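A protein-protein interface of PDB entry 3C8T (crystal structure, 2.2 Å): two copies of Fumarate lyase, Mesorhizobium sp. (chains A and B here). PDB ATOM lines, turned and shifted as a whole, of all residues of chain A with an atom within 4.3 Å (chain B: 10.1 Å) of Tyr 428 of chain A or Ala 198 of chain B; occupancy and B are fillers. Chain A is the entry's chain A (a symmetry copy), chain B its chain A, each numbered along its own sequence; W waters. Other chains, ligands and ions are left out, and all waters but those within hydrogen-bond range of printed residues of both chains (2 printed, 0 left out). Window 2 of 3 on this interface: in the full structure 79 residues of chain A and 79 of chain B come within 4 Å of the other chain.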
ATOM      1  N   LEU A 156     -23.074  17.427  15.176  1.00  0.00           N
ATOM      2  CA  LEU A 156     -22.956  18.672  15.928  1.00  0.00           C
ATOM      3  C   LEU A 156     -22.465  19.736  14.965  1.00  0.00           C
ATOM      4  O   LEU A 156     -22.034  19.404  13.851  1.00  0.00           O
ATOM      5  CB  LEU A 156     -21.966  18.547  17.093  1.00  0.00           C
ATOM      6  CG  LEU A 156     -22.252  17.658  18.316  1.00  0.00           C
ATOM      7  CD1 LEU A 156     -21.084  17.682  19.261  1.00  0.00           C
ATOM      8  CD2 LEU A 156     -23.547  18.049  19.088  1.00  0.00           C
ATOM      9  N   PRO A 157     -22.516  21.027  15.371  1.00  0.00           N
ATOM     10  CA  PRO A 157     -21.909  22.032  14.509  1.00  0.00           C
ATOM     11  C   PRO A 157     -20.384  21.857  14.303  1.00  0.00           C
ATOM     12  O   PRO A 157     -19.674  21.508  15.248  1.00  0.00           O
ATOM     13  CB  PRO A 157     -22.200  23.339  15.255  1.00  0.00           C
ATOM     14  CG  PRO A 157     -23.350  23.024  16.132  1.00  0.00           C
ATOM     15  CD  PRO A 157     -23.145  21.637  16.552  1.00  0.00           C
ATOM     16  N   VAL A 365     -27.957  20.676  18.550  1.00  0.00           N
ATOM     17  CA  VAL A 365     -27.271  21.103  19.784  1.00  0.00           C
ATOM     18  C   VAL A 365     -28.038  20.685  21.085  1.00  0.00           C
ATOM     19  O   VAL A 365     -27.817  21.229  22.183  1.00  0.00           O
ATOM     20  CB  VAL A 365     -26.852  22.618  19.777  1.00  0.00           C
ATOM     21  CG1 VAL A 365     -25.747  22.858  18.725  1.00  0.00           C
ATOM     22  CG2 VAL A 365     -28.054  23.584  19.548  1.00  0.00           C
ATOM     23  N   GLU A 367     -27.186  18.224  22.777  1.00  0.00           N
ATOM     24  CA  GLU A 367     -26.031  17.978  23.668  1.00  0.00           C
ATOM     25  C   GLU A 367     -25.636  19.193  24.538  1.00  0.00           C
ATOM     26  O   GLU A 367     -25.298  19.028  25.714  1.00  0.00           O
ATOM     27  CB  GLU A 367     -24.794  17.530  22.866  1.00  0.00           C
ATOM     28  CG  GLU A 367     -23.721  16.885  23.770  1.00  0.00           C
ATOM     29  CD  GLU A 367     -22.339  16.740  23.096  1.00  0.00           C
ATOM     30  OE1 GLU A 367     -21.932  15.572  22.808  1.00  0.00           O
ATOM     31  OE2 GLU A 367     -21.657  17.785  22.871  1.00  0.00           O
ATOM     32  N   ALA A 368     -25.657  20.398  23.954  1.00  0.00           N
ATOM     33  CA  ALA A 368     -25.374  21.640  24.689  1.00  0.00           C
ATOM     34  C   ALA A 368     -26.379  21.918  25.836  1.00  0.00           C
ATOM     35  O   ALA A 368     -26.005  22.480  26.871  1.00  0.00           O
ATOM     36  CB  ALA A 368     -25.343  22.834  23.727  1.00  0.00           C
ATOM     37  N   MET A 371     -25.366  19.204  28.576  1.00  0.00           N
ATOM     38  CA  MET A 371     -24.163  19.730  29.253  1.00  0.00           C
ATOM     39  C   MET A 371     -24.560  20.787  30.293  1.00  0.00           C
ATOM     40  O   MET A 371     -24.108  20.779  31.431  1.00  0.00           O
ATOM     41  CB  MET A 371     -23.180  20.323  28.212  1.00  0.00           C
ATOM     42  CG  MET A 371     -21.837  20.912  28.748  1.00  0.00           C
ATOM     43  SD  MET A 371     -21.019  22.086  27.608  1.00  0.00           S
ATOM     44  CE  MET A 371     -22.397  23.215  27.282  1.00  0.00           C
ATOM     45  N   PRO A 425     -27.175  26.868  17.309  1.00  0.00           N
ATOM     46  CA  PRO A 425     -25.986  26.074  16.930  1.00  0.00           C
ATOM     47  C   PRO A 425     -24.680  26.874  16.829  1.00  0.00           C
ATOM     48  O   PRO A 425     -23.597  26.320  17.069  1.00  0.00           O
ATOM     49  CB  PRO A 425     -26.395  25.446  15.576  1.00  0.00           C
ATOM     50  CG  PRO A 425     -27.476  26.317  15.075  1.00  0.00           C
ATOM     51  CD  PRO A 425     -28.244  26.746  16.308  1.00  0.00           C
ATOM     52  N   ARG A 426     -24.779  28.168  16.523  1.00  0.00           N
ATOM     53  CA  ARG A 426     -23.574  29.009  16.375  1.00  0.00           C
ATOM     54  C   ARG A 426     -22.775  29.107  17.675  1.00  0.00           C
ATOM     55  O   ARG A 426     -21.579  29.416  17.645  1.00  0.00           O
ATOM     56  CB  ARG A 426     -23.923  30.398  15.827  1.00  0.00           C
ATOM     57  N   ASN A 427     -23.408  28.794  18.807  1.00  0.00           N
ATOM     58  CA  ASN A 427     -22.758  28.881  20.116  1.00  0.00           C
ATOM     59  C   ASN A 427     -22.046  27.616  20.545  1.00  0.00           C
ATOM     60  O   ASN A 427     -21.530  27.566  21.656  1.00  0.00           O
ATOM     61  CB  ASN A 427     -23.754  29.287  21.230  1.00  0.00           C
ATOM     62  CG  ASN A 427     -24.322  30.674  21.010  1.00  0.00           C
ATOM     63  OD1 ASN A 427     -23.607  31.563  20.556  1.00  0.00           O
ATOM     64  ND2 ASN A 427     -25.602  30.862  21.294  1.00  0.00           N
ATOM     65  N   TYR A 428     -22.011  26.592  19.692  1.00  0.00           N
ATOM     66  CA  TYR A 428     -21.481  25.282  20.129  1.00  0.00           C
ATOM     67  C   TYR A 428     -20.406  24.696  19.222  1.00  0.00           C
ATOM     68  O   TYR A 428     -20.555  23.584  18.707  1.00  0.00           O
ATOM     69  CB  TYR A 428     -22.647  24.315  20.259  1.00  0.00           C
ATOM     70  CG  TYR A 428     -22.406  23.172  21.203  1.00  0.00           C
ATOM     71  CD1 TYR A 428     -22.014  23.408  22.511  1.00  0.00           C
ATOM     72  CD2 TYR A 428     -22.586  21.841  20.787  1.00  0.00           C
ATOM     73  CE1 TYR A 428     -21.815  22.367  23.382  1.00  0.00           C
ATOM     74  CE2 TYR A 428     -22.396  20.790  21.663  1.00  0.00           C
ATOM     75  CZ  TYR A 428     -21.998  21.054  22.964  1.00  0.00           C
ATOM     76  OH  TYR A 428     -21.811  20.015  23.884  1.00  0.00           O
ATOM     77  N   LEU A 429     -19.312  25.436  19.043  1.00  0.00           N
ATOM     78  CA  LEU A 429     -18.313  25.077  18.044  1.00  0.00           C
ATOM     79  C   LEU A 429     -17.033  24.545  18.665  1.00  0.00           C
ATOM     80  O   LEU A 429     -16.115  24.087  17.954  1.00  0.00           O
ATOM     81  CB  LEU A 429     -18.046  26.256  17.081  1.00  0.00           C
ATOM     82  CG  LEU A 429     -19.200  26.652  16.115  1.00  0.00           C
ATOM     83  CD1 LEU A 429     -18.866  27.977  15.491  1.00  0.00           C
ATOM     84  CD2 LEU A 429     -19.434  25.587  15.048  1.00  0.00           C
ATOM     85  N   GLY A 430     -16.979  24.589  19.990  1.00  0.00           N
ATOM     86  CA  GLY A 430     -15.946  23.922  20.775  1.00  0.00           C
ATOM     87  C   GLY A 430     -14.548  24.386  20.454  1.00  0.00           C
ATOM     88  O   GLY A 430     -14.266  25.595  20.484  1.00  0.00           O
ATOM     89  N   TRP B 100     -16.398  11.386  29.622  1.00  0.00           N
ATOM     90  CA  TRP B 100     -16.883  12.767  29.739  1.00  0.00           C
ATOM     91  C   TRP B 100     -16.360  13.519  28.549  1.00  0.00           C
ATOM     92  O   TRP B 100     -15.156  13.738  28.440  1.00  0.00           O
ATOM     93  CB  TRP B 100     -16.337  13.367  31.032  1.00  0.00           C
ATOM     94  CG  TRP B 100     -16.809  14.741  31.412  1.00  0.00           C
ATOM     95  CD1 TRP B 100     -16.248  15.950  31.051  1.00  0.00           C
ATOM     96  CD2 TRP B 100     -17.902  15.053  32.275  1.00  0.00           C
ATOM     97  NE1 TRP B 100     -16.949  16.992  31.618  1.00  0.00           N
ATOM     98  CE2 TRP B 100     -17.961  16.470  32.386  1.00  0.00           C
ATOM     99  CE3 TRP B 100     -18.839  14.276  32.967  1.00  0.00           C
ATOM    100  CZ2 TRP B 100     -18.926  17.124  33.167  1.00  0.00           C
ATOM    101  CZ3 TRP B 100     -19.798  14.920  33.741  1.00  0.00           C
ATOM    102  CH2 TRP B 100     -19.828  16.344  33.837  1.00  0.00           C
ATOM    103  N   GLY B 101     -17.254  13.870  27.627  1.00  0.00           N
ATOM    104  CA  GLY B 101     -16.878  14.590  26.419  1.00  0.00           C
ATOM    105  C   GLY B 101     -16.385  13.700  25.285  1.00  0.00           C
ATOM    106  O   GLY B 101     -16.153  14.197  24.195  1.00  0.00           O
ATOM    107  N   ALA B 102     -16.246  12.399  25.555  1.00  0.00           N
ATOM    108  CA  ALA B 102     -15.867  11.369  24.582  1.00  0.00           C
ATOM    109  C   ALA B 102     -17.000  10.940  23.640  1.00  0.00           C
ATOM    110  O   ALA B 102     -18.159  10.954  24.022  1.00  0.00           O
ATOM    111  CB  ALA B 102     -15.330  10.127  25.325  1.00  0.00           C
ATOM    112  N   THR B 103     -16.640  10.546  22.412  1.00  0.00           N
ATOM    113  CA  THR B 103     -17.517   9.777  21.551  1.00  0.00           C
ATOM    114  C   THR B 103     -16.956   8.330  21.420  1.00  0.00           C
ATOM    115  O   THR B 103     -15.784   8.041  21.748  1.00  0.00           O
ATOM    116  CB  THR B 103     -17.744  10.447  20.155  1.00  0.00           C
ATOM    117  OG1 THR B 103     -18.819   9.779  19.464  1.00  0.00           O
ATOM    118  CG2 THR B 103     -16.484  10.364  19.261  1.00  0.00           C
ATOM    119  N   ASP B 106     -13.710   7.747  19.425  1.00  0.00           N
ATOM    120  CA  ASP B 106     -12.517   8.147  20.180  1.00  0.00           C
ATOM    121  C   ASP B 106     -11.941   6.947  20.926  1.00  0.00           C
ATOM    122  O   ASP B 106     -10.761   6.671  20.853  1.00  0.00           O
ATOM    123  CB  ASP B 106     -12.837   9.233  21.187  1.00  0.00           C
ATOM    124  CG  ASP B 106     -13.174  10.536  20.547  1.00  0.00           C
ATOM    125  OD1 ASP B 106     -12.810  10.767  19.370  1.00  0.00           O
ATOM    126  OD2 ASP B 106     -13.798  11.356  21.242  1.00  0.00           O
ATOM    127  N   PHE B 190      -8.950  11.668  20.402  1.00  0.00           N
ATOM    128  CA  PHE B 190      -9.949  12.196  21.328  1.00  0.00           C
ATOM    129  C   PHE B 190     -10.498  13.521  20.818  1.00  0.00           C
ATOM    130  O   PHE B 190      -9.847  14.593  20.966  1.00  0.00           O
ATOM    131  CB  PHE B 190      -9.390  12.348  22.755  1.00  0.00           C
ATOM    132  CG  PHE B 190     -10.422  12.799  23.739  1.00  0.00           C
ATOM    133  CD1 PHE B 190     -11.432  11.927  24.148  1.00  0.00           C
ATOM    134  CD2 PHE B 190     -10.399  14.108  24.231  1.00  0.00           C
ATOM    135  CE1 PHE B 190     -12.405  12.351  25.038  1.00  0.00           C
ATOM    136  CE2 PHE B 190     -11.355  14.558  25.100  1.00  0.00           C
ATOM    137  CZ  PHE B 190     -12.374  13.693  25.527  1.00  0.00           C
ATOM    138  N   SER B 191     -11.665  13.452  20.173  1.00  0.00           N
ATOM    139  CA  SER B 191     -12.224  14.652  19.546  1.00  0.00           C
ATOM    140  C   SER B 191     -13.730  14.780  19.651  1.00  0.00           C
ATOM    141  O   SER B 191     -14.289  15.759  19.189  1.00  0.00           O
ATOM    142  CB  SER B 191     -11.812  14.759  18.074  1.00  0.00           C
ATOM    143  OG  SER B 191     -10.425  15.052  17.941  1.00  0.00           O
ATOM    144  N   GLY B 192     -14.394  13.799  20.230  1.00  0.00           N
ATOM    145  CA  GLY B 192     -15.813  13.915  20.437  1.00  0.00           C
ATOM    146  C   GLY B 192     -16.644  13.728  19.178  1.00  0.00           C
ATOM    147  O   GLY B 192     -16.106  13.476  18.088  1.00  0.00           O
ATOM    148  N   ALA B 193     -17.957  13.920  19.342  1.00  0.00           N
ATOM    149  CA  ALA B 193     -18.991  13.380  18.445  1.00  0.00           C
ATOM    150  C   ALA B 193     -18.841  13.863  17.023  1.00  0.00           C
ATOM    151  O   ALA B 193     -18.940  13.066  16.102  1.00  0.00           O
ATOM    152  CB  ALA B 193     -20.376  13.703  18.970  1.00  0.00           C
ATOM    153  N   SER B 194     -18.570  15.150  16.824  1.00  0.00           N
ATOM    154  CA  SER B 194     -18.220  15.558  15.477  1.00  0.00           C
ATOM    155  C   SER B 194     -16.837  16.162  15.356  1.00  0.00           C
ATOM    156  O   SER B 194     -16.575  16.884  14.411  1.00  0.00           O
ATOM    157  CB  SER B 194     -19.300  16.436  14.808  1.00  0.00           C
ATOM    158  OG  SER B 194     -19.516  17.559  15.608  1.00  0.00           O
ATOM    159  N   GLY B 195     -15.946  15.819  16.275  1.00  0.00           N
ATOM    160  CA  GLY B 195     -14.515  16.167  16.146  1.00  0.00           C
ATOM    161  C   GLY B 195     -14.051  17.527  16.659  1.00  0.00           C
ATOM    162  O   GLY B 195     -12.860  17.881  16.471  1.00  0.00           O
ATOM    163  N   THR B 196     -14.973  18.286  17.273  1.00  0.00           N
ATOM    164  CA  THR B 196     -14.736  19.649  17.791  1.00  0.00           C
ATOM    165  C   THR B 196     -14.606  19.717  19.304  1.00  0.00           C
ATOM    166  O   THR B 196     -14.334  20.807  19.870  1.00  0.00           O
ATOM    167  CB  THR B 196     -15.914  20.616  17.436  1.00  0.00           C
ATOM    168  OG1 THR B 196     -17.153  20.120  17.997  1.00  0.00           O
ATOM    169  CG2 THR B 196     -16.052  20.746  15.933  1.00  0.00           C
ATOM    170  N   LEU B 197     -14.825  18.585  19.989  1.00  0.00           N
ATOM    171  CA  LEU B 197     -14.839  18.597  21.472  1.00  0.00           C
ATOM    172  C   LEU B 197     -15.742  19.728  22.074  1.00  0.00           C
ATOM    173  O   LEU B 197     -15.415  20.330  23.118  1.00  0.00           O
ATOM    174  CB  LEU B 197     -13.387  18.675  22.027  1.00  0.00           C
ATOM    175  CG  LEU B 197     -12.525  17.405  21.820  1.00  0.00           C
ATOM    176  CD1 LEU B 197     -11.077  17.645  22.132  1.00  0.00           C
ATOM    177  CD2 LEU B 197     -13.039  16.190  22.625  1.00  0.00           C
ATOM    178  N   ALA B 198     -16.872  20.011  21.417  1.00  0.00           N
ATOM    179  CA  ALA B 198     -17.765  21.121  21.838  1.00  0.00           C
ATOM    180  C   ALA B 198     -18.185  20.980  23.286  1.00  0.00           C
ATOM    181  O   ALA B 198     -18.231  21.977  24.027  1.00  0.00           O
ATOM    182  CB  ALA B 198     -19.006  21.187  20.965  1.00  0.00           C
ATOM    183  N   SER B 199     -18.490  19.750  23.694  1.00  0.00           N
ATOM    184  CA  SER B 199     -18.962  19.520  25.055  1.00  0.00           C
ATOM    185  C   SER B 199     -17.963  19.893  26.156  1.00  0.00           C
ATOM    186  O   SER B 199     -18.355  19.937  27.315  1.00  0.00           O
ATOM    187  CB  SER B 199     -19.557  18.116  25.233  1.00  0.00           C
ATOM    188  OG  SER B 199     -18.599  17.135  25.462  1.00  0.00           O
ATOM    189  N   LEU B 200     -16.717  20.222  25.777  1.00  0.00           N
ATOM    190  CA  LEU B 200     -15.646  20.569  26.730  1.00  0.00           C
ATOM    191  C   LEU B 200     -15.311  22.069  26.692  1.00  0.00           C
ATOM    192  O   LEU B 200     -14.321  22.546  27.307  1.00  0.00           O
ATOM    193  CB  LEU B 200     -14.383  19.698  26.524  1.00  0.00           C
ATOM    194  CG  LEU B 200     -14.584  18.200  26.841  1.00  0.00           C
ATOM    195  CD1 LEU B 200     -13.399  17.332  26.398  1.00  0.00           C
ATOM    196  CD2 LEU B 200     -14.948  17.939  28.309  1.00  0.00           C
ATOM    197  N   GLY B 201     -16.167  22.804  25.989  1.00  0.00           N
ATOM    198  CA  GLY B 201     -16.068  24.245  25.900  1.00  0.00           C
ATOM    199  C   GLY B 201     -14.765  24.591  25.228  1.00  0.00           C
ATOM    200  O   GLY B 201     -14.563  24.284  24.048  1.00  0.00           O
ATOM    201  N   THR B 202     -13.866  25.194  26.006  1.00  0.00           N
ATOM    202  CA  THR B 202     -12.581  25.687  25.478  1.00  0.00           C
ATOM    203  C   THR B 202     -11.419  24.787  25.882  1.00  0.00           C
ATOM    204  O   THR B 202     -10.298  25.066  25.522  1.00  0.00           O
ATOM    205  CB  THR B 202     -12.250  27.172  25.944  1.00  0.00           C
ATOM    206  OG1 THR B 202     -11.790  27.176  27.310  1.00  0.00           O
ATOM    207  CG2 THR B 202     -13.456  28.104  25.785  1.00  0.00           C
ATOM    208  N   ARG B 203     -11.686  23.723  26.637  1.00  0.00           N
ATOM    209  CA  ARG B 203     -10.602  22.951  27.244  1.00  0.00           C
ATOM    210  C   ARG B 203     -10.264  21.675  26.448  1.00  0.00           C
ATOM    211  O   ARG B 203      -9.390  20.882  26.837  1.00  0.00           O
ATOM    212  CB  ARG B 203     -10.955  22.589  28.698  1.00  0.00           C
ATOM    213  CG  ARG B 203     -11.450  23.743  29.586  1.00  0.00           C
ATOM    214  CD  ARG B 203     -10.335  24.687  30.009  1.00  0.00           C
ATOM    215  NE  ARG B 203      -9.063  24.021  30.336  1.00  0.00           N
ATOM    216  CZ  ARG B 203      -8.787  23.465  31.521  1.00  0.00           C
ATOM    217  NH1 ARG B 203      -7.598  22.909  31.731  1.00  0.00           N
ATOM    218  NH2 ARG B 203      -9.700  23.454  32.491  1.00  0.00           N
ATOM    219  N   GLY B 204     -10.949  21.473  25.338  1.00  0.00           N
ATOM    220  CA  GLY B 204     -10.801  20.220  24.585  1.00  0.00           C
ATOM    221  C   GLY B 204      -9.386  19.806  24.219  1.00  0.00           C
ATOM    222  O   GLY B 204      -8.989  18.680  24.475  1.00  0.00           O
ATOM    223  N   LEU B 205      -8.622  20.718  23.632  1.00  0.00           N
ATOM    224  CA  LEU B 205      -7.235  20.405  23.211  1.00  0.00           C
ATOM    225  C   LEU B 205      -6.285  20.079  24.388  1.00  0.00           C
ATOM    226  O   LEU B 205      -5.362  19.263  24.235  1.00  0.00           O
ATOM    227  CB  LEU B 205      -6.675  21.524  22.356  1.00  0.00           C
ATOM    228  CG  LEU B 205      -6.942  21.455  20.845  1.00  0.00           C
ATOM    229  CD1 LEU B 205      -8.376  21.348  20.587  1.00  0.00           C
ATOM    230  CD2 LEU B 205      -6.466  22.704  20.145  1.00  0.00           C
ATOM    231  N   THR B 223      -8.154  15.928  14.636  1.00  0.00           N
ATOM    232  CA  THR B 223      -9.096  14.825  14.550  1.00  0.00           C
ATOM    233  C   THR B 223      -8.863  13.959  13.310  1.00  0.00           C
ATOM    234  O   THR B 223      -8.725  14.469  12.173  1.00  0.00           O
ATOM    235  CB  THR B 223     -10.530  15.399  14.510  1.00  0.00           C
ATOM    236  OG1 THR B 223     -10.689  16.309  15.600  1.00  0.00           O
ATOM    237  CG2 THR B 223     -11.609  14.272  14.585  1.00  0.00           C
ATOM    238  N   HIS B 225     -10.893  11.020  12.804  1.00  0.00           N
ATOM    239  CA  HIS B 225     -12.070  10.156  12.667  1.00  0.00           C
ATOM    240  C   HIS B 225     -12.243   9.801  11.179  1.00  0.00           C
ATOM    241  O   HIS B 225     -12.604   8.672  10.850  1.00  0.00           O
ATOM    242  CB  HIS B 225     -13.336  10.856  13.168  1.00  0.00           C
ATOM    243  CG  HIS B 225     -13.418  11.019  14.660  1.00  0.00           C
ATOM    244  ND1 HIS B 225     -14.119  12.052  15.255  1.00  0.00           N
ATOM    245  CD2 HIS B 225     -12.907  10.287  15.672  1.00  0.00           C
ATOM    246  CE1 HIS B 225     -14.024  11.950  16.565  1.00  0.00           C
ATOM    247  NE2 HIS B 225     -13.305  10.878  16.845  1.00  0.00           N
HETATM  248  O   HOH W   1     -20.181  14.548  25.119  1.00  0.00           O
HETATM  249  O   HOH W   2     -19.301  21.398  17.760  1.00  0.00           O
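SD of Met 371 of chain A sits close to O of Ser 199 of chain B. The backbone NH (N) of Ser 199 of chain B sits close to the side-chain hydroxyl (OH) of Tyr 428 of chain A, 3.3 Å away.
The side-chain hydroxyl of Thr 196 of chain B sits close to the backbone NH of Ala 198 of chain B, at 3.4 Å. OE2 of Glu 367 of chain A is in hydrogen-bond range of OH of Tyr 428 of chain A (2.5 Å). The backbone carbonyl oxygen (O) of Ser 191 of chain B is in hydrogen-bond range of the backbone NH (N) of Thr 196 of chain B.
CB of Leu 156 of chain A touches OG of Ser 194 of chain B, 3.0 Å away. O of Pro 157 of chain A touches OG of Ser 194 of chain B, at 3.97 Å. Pro 157 of chain A touches Thr 196 of chain B (O to CG2, 3.8 Å). Glu 367 of chain A touches Ser 199 of chain B. Tyr 428 of chain A touches Ala 198 of chain B (CE2 to CB, 3.5 Å). O of Leu 429 of chain A touches CB of Thr 196 of chain B, at 3.5 Å. Gly 430 of chain A touches Thr 196 of chain B. CA of Gly 430 of chain A touches CA of Ala 198 of chain B, 3.5 Å away. CA of Gly 430 of chain A touches O of Gly 201 of chain B, at 3.6 Å.
Of the printed residues of chain B, Leu 156 of chain A touches Ser 194. Glu 367 of chain A touches just one residue of chain B: Ser 199 (3.2 Å). No residue of chain B comes within 4 Å of Ala 368 of chain A. Printed residues of chain B within 4 Å of Met 371 of chain A: Ser 199. No residue of chain B comes within 4 Å of Arg 426 of chain A. Gly 430 of chain A touches just these residues of chain B: Thr 196, Ala 198 and Gly 201. Ala 102 of chain B touches none of the printed residues of chain A. Thr 103 of chain B touches none of the printed residues of chain A. Of the printed residues of chain A, Thr 196 of chain B touches Pro 157 (3.8 Å), Leu 429 (3.5 Å) and Gly 430 (3.6 Å). Ala 198 of chain B touches two residues of chain A. Of the printed residues of chain A, Ser 199 of chain B touches Glu 367, Met 371 and Tyr 428. Printed residues of chain A within 4 Å of Gly 201 of chain B: Gly 430. The nearest residue of chain B that does not touch Tyr 428 of chain A is Thr 196 of chain B (4.9 Å). The nearest printed residue of chain B that does not touch Leu 156 of chain A is Ala 193 of chain B (4.1 Å).
Hydrophobic or aromatic side chains of chain B within 4 Å of the printed part of chain A: Ala 198.
No position is printed for both chains.
Water W2 lies within hydrogen-bond range of OG1 of Thr 196 of chain B (2.5 Å), O of Pro 157 of chain A (2.5 Å) and O of Tyr 428 of chain A (2.7 Å). Water W1 bridges the side-chain hydroxyl (OG) of Ser 199 of chain B and the side-chain carboxylate (OE1) of Glu 367 of chain A.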
